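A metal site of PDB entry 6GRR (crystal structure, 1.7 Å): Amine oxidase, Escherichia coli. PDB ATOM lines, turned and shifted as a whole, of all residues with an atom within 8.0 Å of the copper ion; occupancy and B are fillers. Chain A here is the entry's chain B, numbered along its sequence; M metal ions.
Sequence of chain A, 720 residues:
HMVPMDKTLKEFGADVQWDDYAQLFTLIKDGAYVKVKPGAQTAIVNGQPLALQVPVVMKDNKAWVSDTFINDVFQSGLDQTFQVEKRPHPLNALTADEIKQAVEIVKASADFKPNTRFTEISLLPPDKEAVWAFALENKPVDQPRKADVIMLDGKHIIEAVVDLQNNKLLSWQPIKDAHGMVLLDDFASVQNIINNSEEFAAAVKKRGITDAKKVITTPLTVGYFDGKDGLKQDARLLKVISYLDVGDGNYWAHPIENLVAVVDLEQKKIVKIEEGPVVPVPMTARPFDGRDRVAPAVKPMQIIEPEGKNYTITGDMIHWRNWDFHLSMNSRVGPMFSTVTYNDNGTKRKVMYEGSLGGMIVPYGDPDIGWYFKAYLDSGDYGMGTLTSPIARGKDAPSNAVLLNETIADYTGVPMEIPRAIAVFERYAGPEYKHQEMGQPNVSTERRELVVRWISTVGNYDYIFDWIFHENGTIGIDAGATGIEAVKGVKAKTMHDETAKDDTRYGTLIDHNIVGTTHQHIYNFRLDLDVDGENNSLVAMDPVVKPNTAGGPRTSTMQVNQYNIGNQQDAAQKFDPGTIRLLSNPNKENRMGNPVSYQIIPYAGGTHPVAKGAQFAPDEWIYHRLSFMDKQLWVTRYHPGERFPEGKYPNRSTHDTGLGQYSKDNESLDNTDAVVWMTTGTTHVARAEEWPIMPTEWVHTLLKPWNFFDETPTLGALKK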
ATOM      1  N   VAL A 362       9.043   8.413  28.454  1.00  0.00           N
ATOM      2  CA  VAL A 362       8.016   8.252  27.436  1.00  0.00           C
ATOM      3  C   VAL A 362       8.380   9.107  26.223  1.00  0.00           C
ATOM      4  O   VAL A 362       8.001  10.286  26.168  1.00  0.00           O
ATOM      5  CB  VAL A 362       6.657   8.628  28.014  1.00  0.00           C
ATOM      6  CG1 VAL A 362       5.548   8.434  27.000  1.00  0.00           C
ATOM      7  CG2 VAL A 362       6.365   7.805  29.263  1.00  0.00           C
ATOM      8  N   TYR A 364       8.420  10.108  22.083  1.00  0.00           N
ATOM      9  CA  TYR A 364       7.506  10.075  20.949  1.00  0.00           C
ATOM     10  C   TYR A 364       8.204   9.895  19.611  1.00  0.00           C
ATOM     11  O   TYR A 364       9.416  10.030  19.512  1.00  0.00           O
ATOM     12  CB  TYR A 364       6.642  11.322  20.970  1.00  0.00           C
ATOM     13  CG  TYR A 364       5.602  11.206  22.055  1.00  0.00           C
ATOM     14  CD1 TYR A 364       5.924  11.430  23.400  1.00  0.00           C
ATOM     15  CD2 TYR A 364       4.305  10.825  21.743  1.00  0.00           C
ATOM     16  CE1 TYR A 364       4.963  11.253  24.382  1.00  0.00           C
ATOM     17  CE2 TYR A 364       3.355  10.663  22.718  1.00  0.00           C
ATOM     18  CZ  TYR A 364       3.688  10.864  24.030  1.00  0.00           C
ATOM     19  OH  TYR A 364       2.681  10.694  24.960  1.00  0.00           O
ATOM     20  N   ASN A 460      -0.565  14.221  31.447  1.00  0.00           N
ATOM     21  CA  ASN A 460      -1.691  13.455  30.860  1.00  0.00           C
ATOM     22  C   ASN A 460      -1.733  11.991  31.332  1.00  0.00           C
ATOM     23  O   ASN A 460      -2.793  11.398  31.394  1.00  0.00           O
ATOM     24  CB  ASN A 460      -1.666  13.502  29.322  1.00  0.00           C
ATOM     25  CG  ASN A 460      -0.354  13.018  28.749  1.00  0.00           C
ATOM     26  OD1 ASN A 460       0.684  13.610  29.024  1.00  0.00           O
ATOM     27  ND2 ASN A 460      -0.370  11.909  27.994  1.00  0.00           N
ATOM     28  N   TYR A 461      -0.575  11.437  31.682  1.00  0.00           N
ATOM     29  CA  TYR A 461      -0.481  10.019  32.006  1.00  0.00           C
ATOM     30  C   TYR A 461      -0.405   9.743  33.506  1.00  0.00           C
ATOM     31  O   TYR A 461       0.176  10.526  34.251  1.00  0.00           O
ATOM     32  CB  TYR A 461       0.730   9.397  31.294  1.00  0.00           C
ATOM     33  CG  TYR A 461       0.461   8.773  29.915  1.00  0.00           C
ATOM     34  CD1 TYR A 461      -0.696   8.056  29.643  1.00  0.00           C
ATOM     35  CD2 TYR A 461       1.415   8.863  28.900  1.00  0.00           C
ATOM     36  CE1 TYR A 461      -0.932   7.457  28.400  1.00  0.00           C
ATOM     37  CE2 TYR A 461       1.183   8.258  27.651  1.00  0.00           C
ATOM     38  CZ  TYR A 461       0.029   7.546  27.422  1.00  0.00           C
ATOM     39  OH  TYR A 461      -0.212   6.941  26.212  1.00  0.00           O
ATOM     40  N   TYR A 463       0.703   6.677  36.225  1.00  0.00           N
ATOM     41  CA  TYR A 463       1.500   5.461  36.314  1.00  0.00           C
ATOM     42  C   TYR A 463       1.280   4.796  37.649  1.00  0.00           C
ATOM     43  O   TYR A 463       1.243   5.466  38.668  1.00  0.00           O
ATOM     44  CB  TYR A 463       2.973   5.777  36.120  1.00  0.00           C
ATOM     45  CG  TYR A 463       3.223   6.373  34.763  1.00  0.00           C
ATOM     46  CD1 TYR A 463       3.160   5.566  33.634  1.00  0.00           C
ATOM     47  CD2 TYR A 463       3.442   7.739  34.595  1.00  0.00           C
ATOM     48  CE1 TYR A 463       3.351   6.087  32.365  1.00  0.00           C
ATOM     49  CE2 TYR A 463       3.647   8.270  33.313  1.00  0.00           C
ATOM     50  CZ  TYR A 463       3.592   7.424  32.225  1.00  0.00           C
ATOM     51  OH  TYR A 463       3.753   7.889  30.927  1.00  0.00           O
ATOM     52  N   ALA A 481      -0.071   1.697  33.216  1.00  0.00           N
ATOM     53  CA  ALA A 481      -0.221   3.041  32.646  1.00  0.00           C
ATOM     54  C   ALA A 481      -1.656   3.237  32.285  1.00  0.00           C
ATOM     55  O   ALA A 481      -2.272   2.342  31.726  1.00  0.00           O
ATOM     56  CB  ALA A 481       0.664   3.202  31.427  1.00  0.00           C
ATOM     57  N   THR A 482      -2.184   4.392  32.637  1.00  0.00           N
ATOM     58  CA  THR A 482      -3.552   4.787  32.275  1.00  0.00           C
ATOM     59  C   THR A 482      -3.514   6.315  32.108  1.00  0.00           C
ATOM     60  O   THR A 482      -2.440   6.890  32.026  1.00  0.00           O
ATOM     61  CB  THR A 482      -4.597   4.272  33.299  1.00  0.00           C
ATOM     62  OG1 THR A 482      -5.916   4.676  32.916  1.00  0.00           O
ATOM     63  CG2 THR A 482      -4.291   4.725  34.725  1.00  0.00           C
ATOM     64  N   ILE A 484      -4.696   9.872  29.845  1.00  0.00           N
ATOM     65  CA  ILE A 484      -5.233  10.455  28.613  1.00  0.00           C
ATOM     66  C   ILE A 484      -4.069  10.478  27.623  1.00  0.00           C
ATOM     67  O   ILE A 484      -2.974  10.902  27.955  1.00  0.00           O
ATOM     68  CB  ILE A 484      -5.770  11.897  28.786  1.00  0.00           C
ATOM     69  CG1 ILE A 484      -6.635  12.044  30.055  1.00  0.00           C
ATOM     70  CG2 ILE A 484      -6.568  12.335  27.554  1.00  0.00           C
ATOM     71  CD1 ILE A 484      -7.812  11.104  30.174  1.00  0.00           C
ATOM     72  N   GLU A 485      -4.316   9.990  26.407  1.00  0.00           N
ATOM     73  CA  GLU A 485      -3.309   9.994  25.341  1.00  0.00           C
ATOM     74  C   GLU A 485      -2.890  11.425  24.992  1.00  0.00           C
ATOM     75  O   GLU A 485      -3.694  12.345  25.067  1.00  0.00           O
ATOM     76  CB  GLU A 485      -3.890   9.339  24.080  1.00  0.00           C
ATOM     77  CG  GLU A 485      -4.061   7.842  24.173  1.00  0.00           C
ATOM     78  CD  GLU A 485      -2.813   7.159  24.689  1.00  0.00           C
ATOM     79  OE1 GLU A 485      -1.815   7.079  23.939  1.00  0.00           O
ATOM     80  OE2 GLU A 485      -2.843   6.720  25.869  1.00  0.00           O
ATOM     81  N   ALA A 486      -1.623  11.585  24.603  1.00  0.00           N
ATOM     82  CA  ALA A 486      -1.142  12.825  23.984  1.00  0.00           C
ATOM     83  C   ALA A 486      -1.473  12.699  22.497  1.00  0.00           C
ATOM     84  O   ALA A 486      -0.990  11.785  21.813  1.00  0.00           O
ATOM     85  CB  ALA A 486       0.340  12.961  24.178  1.00  0.00           C
ATOM     86  N   THR A 517      -0.406   9.664  18.681  1.00  0.00           N
ATOM     87  CA  THR A 517       0.946   9.533  18.207  1.00  0.00           C
ATOM     88  C   THR A 517       1.708   8.400  18.881  1.00  0.00           C
ATOM     89  O   THR A 517       1.726   8.312  20.106  1.00  0.00           O
ATOM     90  CB  THR A 517       1.702  10.841  18.464  1.00  0.00           C
ATOM     91  OG1 THR A 517       0.974  11.925  17.875  1.00  0.00           O
ATOM     92  CG2 THR A 517       3.078  10.781  17.895  1.00  0.00           C
ATOM     93  N   THR A 518       2.325   7.544  18.068  1.00  0.00           N
ATOM     94  CA  THR A 518       3.098   6.399  18.562  1.00  0.00           C
ATOM     95  C   THR A 518       4.253   6.847  19.433  1.00  0.00           C
ATOM     96  O   THR A 518       4.891   7.884  19.172  1.00  0.00           O
ATOM     97  CB  THR A 518       3.621   5.510  17.393  1.00  0.00           C
ATOM     98  OG1 THR A 518       2.504   5.059  16.629  1.00  0.00           O
ATOM     99  CG2 THR A 518       4.410   4.315  17.885  1.00  0.00           C
ATOM    100  N   HIS A 519       4.505   6.080  20.486  1.00  0.00           N
ATOM    101  CA  HIS A 519       5.545   6.409  21.464  1.00  0.00           C
ATOM    102  C   HIS A 519       5.878   5.139  22.244  1.00  0.00           C
ATOM    103  O   HIS A 519       5.296   4.099  22.012  1.00  0.00           O
ATOM    104  CB  HIS A 519       5.018   7.503  22.394  1.00  0.00           C
ATOM    105  CG  HIS A 519       3.761   7.110  23.082  1.00  0.00           C
ATOM    106  ND1 HIS A 519       2.535   7.129  22.448  1.00  0.00           N
ATOM    107  CD2 HIS A 519       3.551   6.583  24.311  1.00  0.00           C
ATOM    108  CE1 HIS A 519       1.612   6.678  23.283  1.00  0.00           C
ATOM    109  NE2 HIS A 519       2.203   6.337  24.420  1.00  0.00           N
ATOM    110  N   GLN A 520       6.853   5.220  23.147  1.00  0.00           N
ATOM    111  CA  GLN A 520       7.185   4.100  24.002  1.00  0.00           C
ATOM    112  C   GLN A 520       6.948   4.483  25.454  1.00  0.00           C
ATOM    113  O   GLN A 520       6.921   5.660  25.782  1.00  0.00           O
ATOM    114  CB  GLN A 520       8.618   3.702  23.801  1.00  0.00           C
ATOM    115  CG  GLN A 520       8.919   3.150  22.412  1.00  0.00           C
ATOM    116  CD  GLN A 520      10.333   2.639  22.333  1.00  0.00           C
ATOM    117  OE1 GLN A 520      11.287   3.413  22.197  1.00  0.00           O
ATOM    118  NE2 GLN A 520      10.483   1.349  22.455  1.00  0.00           N
ATOM    119  N   HIS A 521       6.746   3.495  26.306  1.00  0.00           N
ATOM    120  CA  HIS A 521       6.806   3.688  27.759  1.00  0.00           C
ATOM    121  C   HIS A 521       7.938   2.846  28.235  1.00  0.00           C
ATOM    122  O   HIS A 521       7.890   1.624  28.066  1.00  0.00           O
ATOM    123  CB  HIS A 521       5.522   3.242  28.462  1.00  0.00           C
ATOM    124  CG  HIS A 521       4.290   3.988  28.021  1.00  0.00           C
ATOM    125  ND1 HIS A 521       3.830   5.112  28.664  1.00  0.00           N
ATOM    126  CD2 HIS A 521       3.453   3.767  26.991  1.00  0.00           C
ATOM    127  CE1 HIS A 521       2.733   5.536  28.064  1.00  0.00           C
ATOM    128  NE2 HIS A 521       2.484   4.733  27.032  1.00  0.00           N
ATOM    129  N   TYR A 523      10.389   1.910  31.481  1.00  0.00           N
ATOM    130  CA  TYR A 523      10.611   1.987  32.923  1.00  0.00           C
ATOM    131  C   TYR A 523      11.918   1.325  33.231  1.00  0.00           C
ATOM    132  O   TYR A 523      12.290   0.337  32.616  1.00  0.00           O
ATOM    133  CB  TYR A 523       9.507   1.255  33.695  1.00  0.00           C
ATOM    134  CG  TYR A 523       8.128   1.582  33.251  1.00  0.00           C
ATOM    135  CD1 TYR A 523       7.448   2.668  33.792  1.00  0.00           C
ATOM    136  CD2 TYR A 523       7.487   0.820  32.292  1.00  0.00           C
ATOM    137  CE1 TYR A 523       6.157   2.975  33.381  1.00  0.00           C
ATOM    138  CE2 TYR A 523       6.209   1.132  31.854  1.00  0.00           C
ATOM    139  CZ  TYR A 523       5.529   2.205  32.422  1.00  0.00           C
ATOM    140  OH  TYR A 523       4.251   2.518  31.985  1.00  0.00           O
ATOM    141  N   HIS A 608       0.693  -4.478  26.278  1.00  0.00           N
ATOM    142  CA  HIS A 608       1.007  -3.735  25.027  1.00  0.00           C
ATOM    143  C   HIS A 608       2.172  -4.449  24.354  1.00  0.00           C
ATOM    144  O   HIS A 608       2.882  -5.243  25.013  1.00  0.00           O
ATOM    145  CB  HIS A 608       1.410  -2.267  25.304  1.00  0.00           C
ATOM    146  CG  HIS A 608       0.291  -1.284  25.272  1.00  0.00           C
ATOM    147  ND1 HIS A 608       0.363  -0.081  25.949  1.00  0.00           N
ATOM    148  CD2 HIS A 608      -0.908  -1.287  24.631  1.00  0.00           C
ATOM    149  CE1 HIS A 608      -0.740   0.619  25.716  1.00  0.00           C
ATOM    150  NE2 HIS A 608      -1.544  -0.102  24.943  1.00  0.00           N
ATOM    151  N   THR A 682       7.397  -0.721  26.491  1.00  0.00           N
ATOM    152  CA  THR A 682       6.384  -1.086  25.534  1.00  0.00           C
ATOM    153  C   THR A 682       6.481  -0.107  24.389  1.00  0.00           C
ATOM    154  O   THR A 682       7.038   0.994  24.547  1.00  0.00           O
ATOM    155  CB  THR A 682       4.969  -0.995  26.109  1.00  0.00           C
ATOM    156  OG1 THR A 682       4.689   0.338  26.544  1.00  0.00           O
ATOM    157  CG2 THR A 682       4.819  -1.926  27.280  1.00  0.00           C
ATOM    158  N   THR A 683       5.916  -0.522  23.252  1.00  0.00           N
ATOM    159  CA  THR A 683       5.732   0.345  22.124  1.00  0.00           C
ATOM    160  C   THR A 683       4.247   0.508  21.986  1.00  0.00           C
ATOM    161  O   THR A 683       3.542  -0.462  21.696  1.00  0.00           O
ATOM    162  CB  THR A 683       6.357  -0.232  20.828  1.00  0.00           C
ATOM    163  OG1 THR A 683       7.779  -0.261  20.996  1.00  0.00           O
ATOM    164  CG2 THR A 683       6.038   0.649  19.639  1.00  0.00           C
ATOM    165  N   HIS A 684       3.776   1.733  22.207  1.00  0.00           N
ATOM    166  CA  HIS A 684       2.377   2.002  22.261  1.00  0.00           C
ATOM    167  C   HIS A 684       1.872   2.555  20.926  1.00  0.00           C
ATOM    168  O   HIS A 684       2.012   3.741  20.643  1.00  0.00           O
ATOM    169  CB  HIS A 684       2.044   2.995  23.403  1.00  0.00           C
ATOM    170  CG  HIS A 684       0.580   3.221  23.605  1.00  0.00           C
ATOM    171  ND1 HIS A 684       0.067   4.033  24.592  1.00  0.00           N
ATOM    172  CD2 HIS A 684      -0.500   2.724  22.938  1.00  0.00           C
ATOM    173  CE1 HIS A 684      -1.256   4.045  24.508  1.00  0.00           C
ATOM    174  NE2 HIS A 684      -1.626   3.253  23.519  1.00  0.00           N
ATOM    175  N   VAL A 685       1.227   1.678  20.163  1.00  0.00           N
ATOM    176  CA  VAL A 685       0.470   2.051  18.990  1.00  0.00           C
ATOM    177  C   VAL A 685      -0.977   2.105  19.439  1.00  0.00           C
ATOM    178  O   VAL A 685      -1.524   1.133  20.008  1.00  0.00           O
ATOM    179  CB  VAL A 685       0.658   1.047  17.835  1.00  0.00           C
ATOM    180  CG1 VAL A 685      -0.270   1.407  16.662  1.00  0.00           C
ATOM    181  CG2 VAL A 685       2.105   0.993  17.416  1.00  0.00           C
ATOM    182  N   ALA A 686      -1.609   3.248  19.181  1.00  0.00           N
ATOM    183  CA  ALA A 686      -2.921   3.528  19.758  1.00  0.00           C
ATOM    184  C   ALA A 686      -4.086   2.905  19.027  1.00  0.00           C
ATOM    185  O   ALA A 686      -3.993   2.503  17.859  1.00  0.00           O
ATOM    186  CB  ALA A 686      -3.124   5.047  19.892  1.00  0.00           C
ATOM    187  N   GLU A 690      -8.848   3.210  23.465  1.00  0.00           N
ATOM    188  CA  GLU A 690      -8.001   3.923  24.458  1.00  0.00           C
ATOM    189  C   GLU A 690      -8.329   5.407  24.553  1.00  0.00           C
ATOM    190  O   GLU A 690      -7.612   6.164  25.218  1.00  0.00           O
ATOM    191  CB  GLU A 690      -6.525   3.687  24.137  1.00  0.00           C
ATOM    192  CG  GLU A 690      -6.120   2.193  24.135  1.00  0.00           C
ATOM    193  CD  GLU A 690      -4.714   1.926  23.611  1.00  0.00           C
ATOM    194  OE1 GLU A 690      -4.165   2.772  22.885  1.00  0.00           O
ATOM    195  OE2 GLU A 690      -4.147   0.839  23.894  1.00  0.00           O
ATOM    196  N   MET A 694      -7.561   5.887  28.612  1.00  0.00           N
ATOM    197  CA  MET A 694      -6.921   4.595  28.325  1.00  0.00           C
ATOM    198  C   MET A 694      -7.115   3.560  29.455  1.00  0.00           C
ATOM    199  O   MET A 694      -6.671   3.795  30.583  1.00  0.00           O
ATOM    200  CB  MET A 694      -5.430   4.797  28.081  1.00  0.00           C
ATOM    201  CG  MET A 694      -4.721   3.483  27.878  1.00  0.00           C
ATOM    202  SD  MET A 694      -3.027   3.552  27.333  1.00  0.00           S
ATOM    203  CE  MET A 694      -2.220   4.116  28.819  1.00  0.00           C
ATOM    204  N   GLU A 697      -3.012  -0.500  31.220  1.00  0.00           N
ATOM    205  CA  GLU A 697      -2.191  -1.494  30.553  1.00  0.00           C
ATOM    206  C   GLU A 697      -1.006  -1.782  31.500  1.00  0.00           C
ATOM    207  O   GLU A 697      -0.533  -0.882  32.170  1.00  0.00           O
ATOM    208  CB  GLU A 697      -1.685  -0.936  29.239  1.00  0.00           C
ATOM    209  CG  GLU A 697      -2.814  -0.590  28.247  1.00  0.00           C
ATOM    210  CD  GLU A 697      -3.278  -1.770  27.401  1.00  0.00           C
ATOM    211  OE1 GLU A 697      -2.817  -2.926  27.628  1.00  0.00           O
ATOM    212  OE2 GLU A 697      -4.153  -1.540  26.507  1.00  0.00           O
HETATM  213 CU    CU M   1       1.141   5.338  25.804  1.00  0.00          CU
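The backbone carbonyl oxygen of His 521 lies within hydrogen-bond range of the backbone NH of Thr 682 (2.9 Å).
A ring nitrogen (ND1) of His 519 is in hydrogen-bond range of the backbone carbonyl oxygen (O) of Thr 517, 2.7 Å away.
NE2 of His 684 sits at hydrogen-bond distance from OE1 of Glu 690, 2.7 Å away.
OE2 of Glu 485 sits close to OH of Tyr 461 (2.7 Å).
The copper ion is bound by a ring nitrogen (NE2) of His 521, a ring nitrogen (NE2) of His 519, a ring nitrogen (ND1) of His 684 and the side-chain hydroxyl (OH) of Tyr 461.
The copper ion has four donor atoms within binding distance.
Residues that only touch the copper ion: Glu 485.
Within 4 Å of the copper ion: Tyr 461, Glu 485, His 519, His 521 and His 684.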
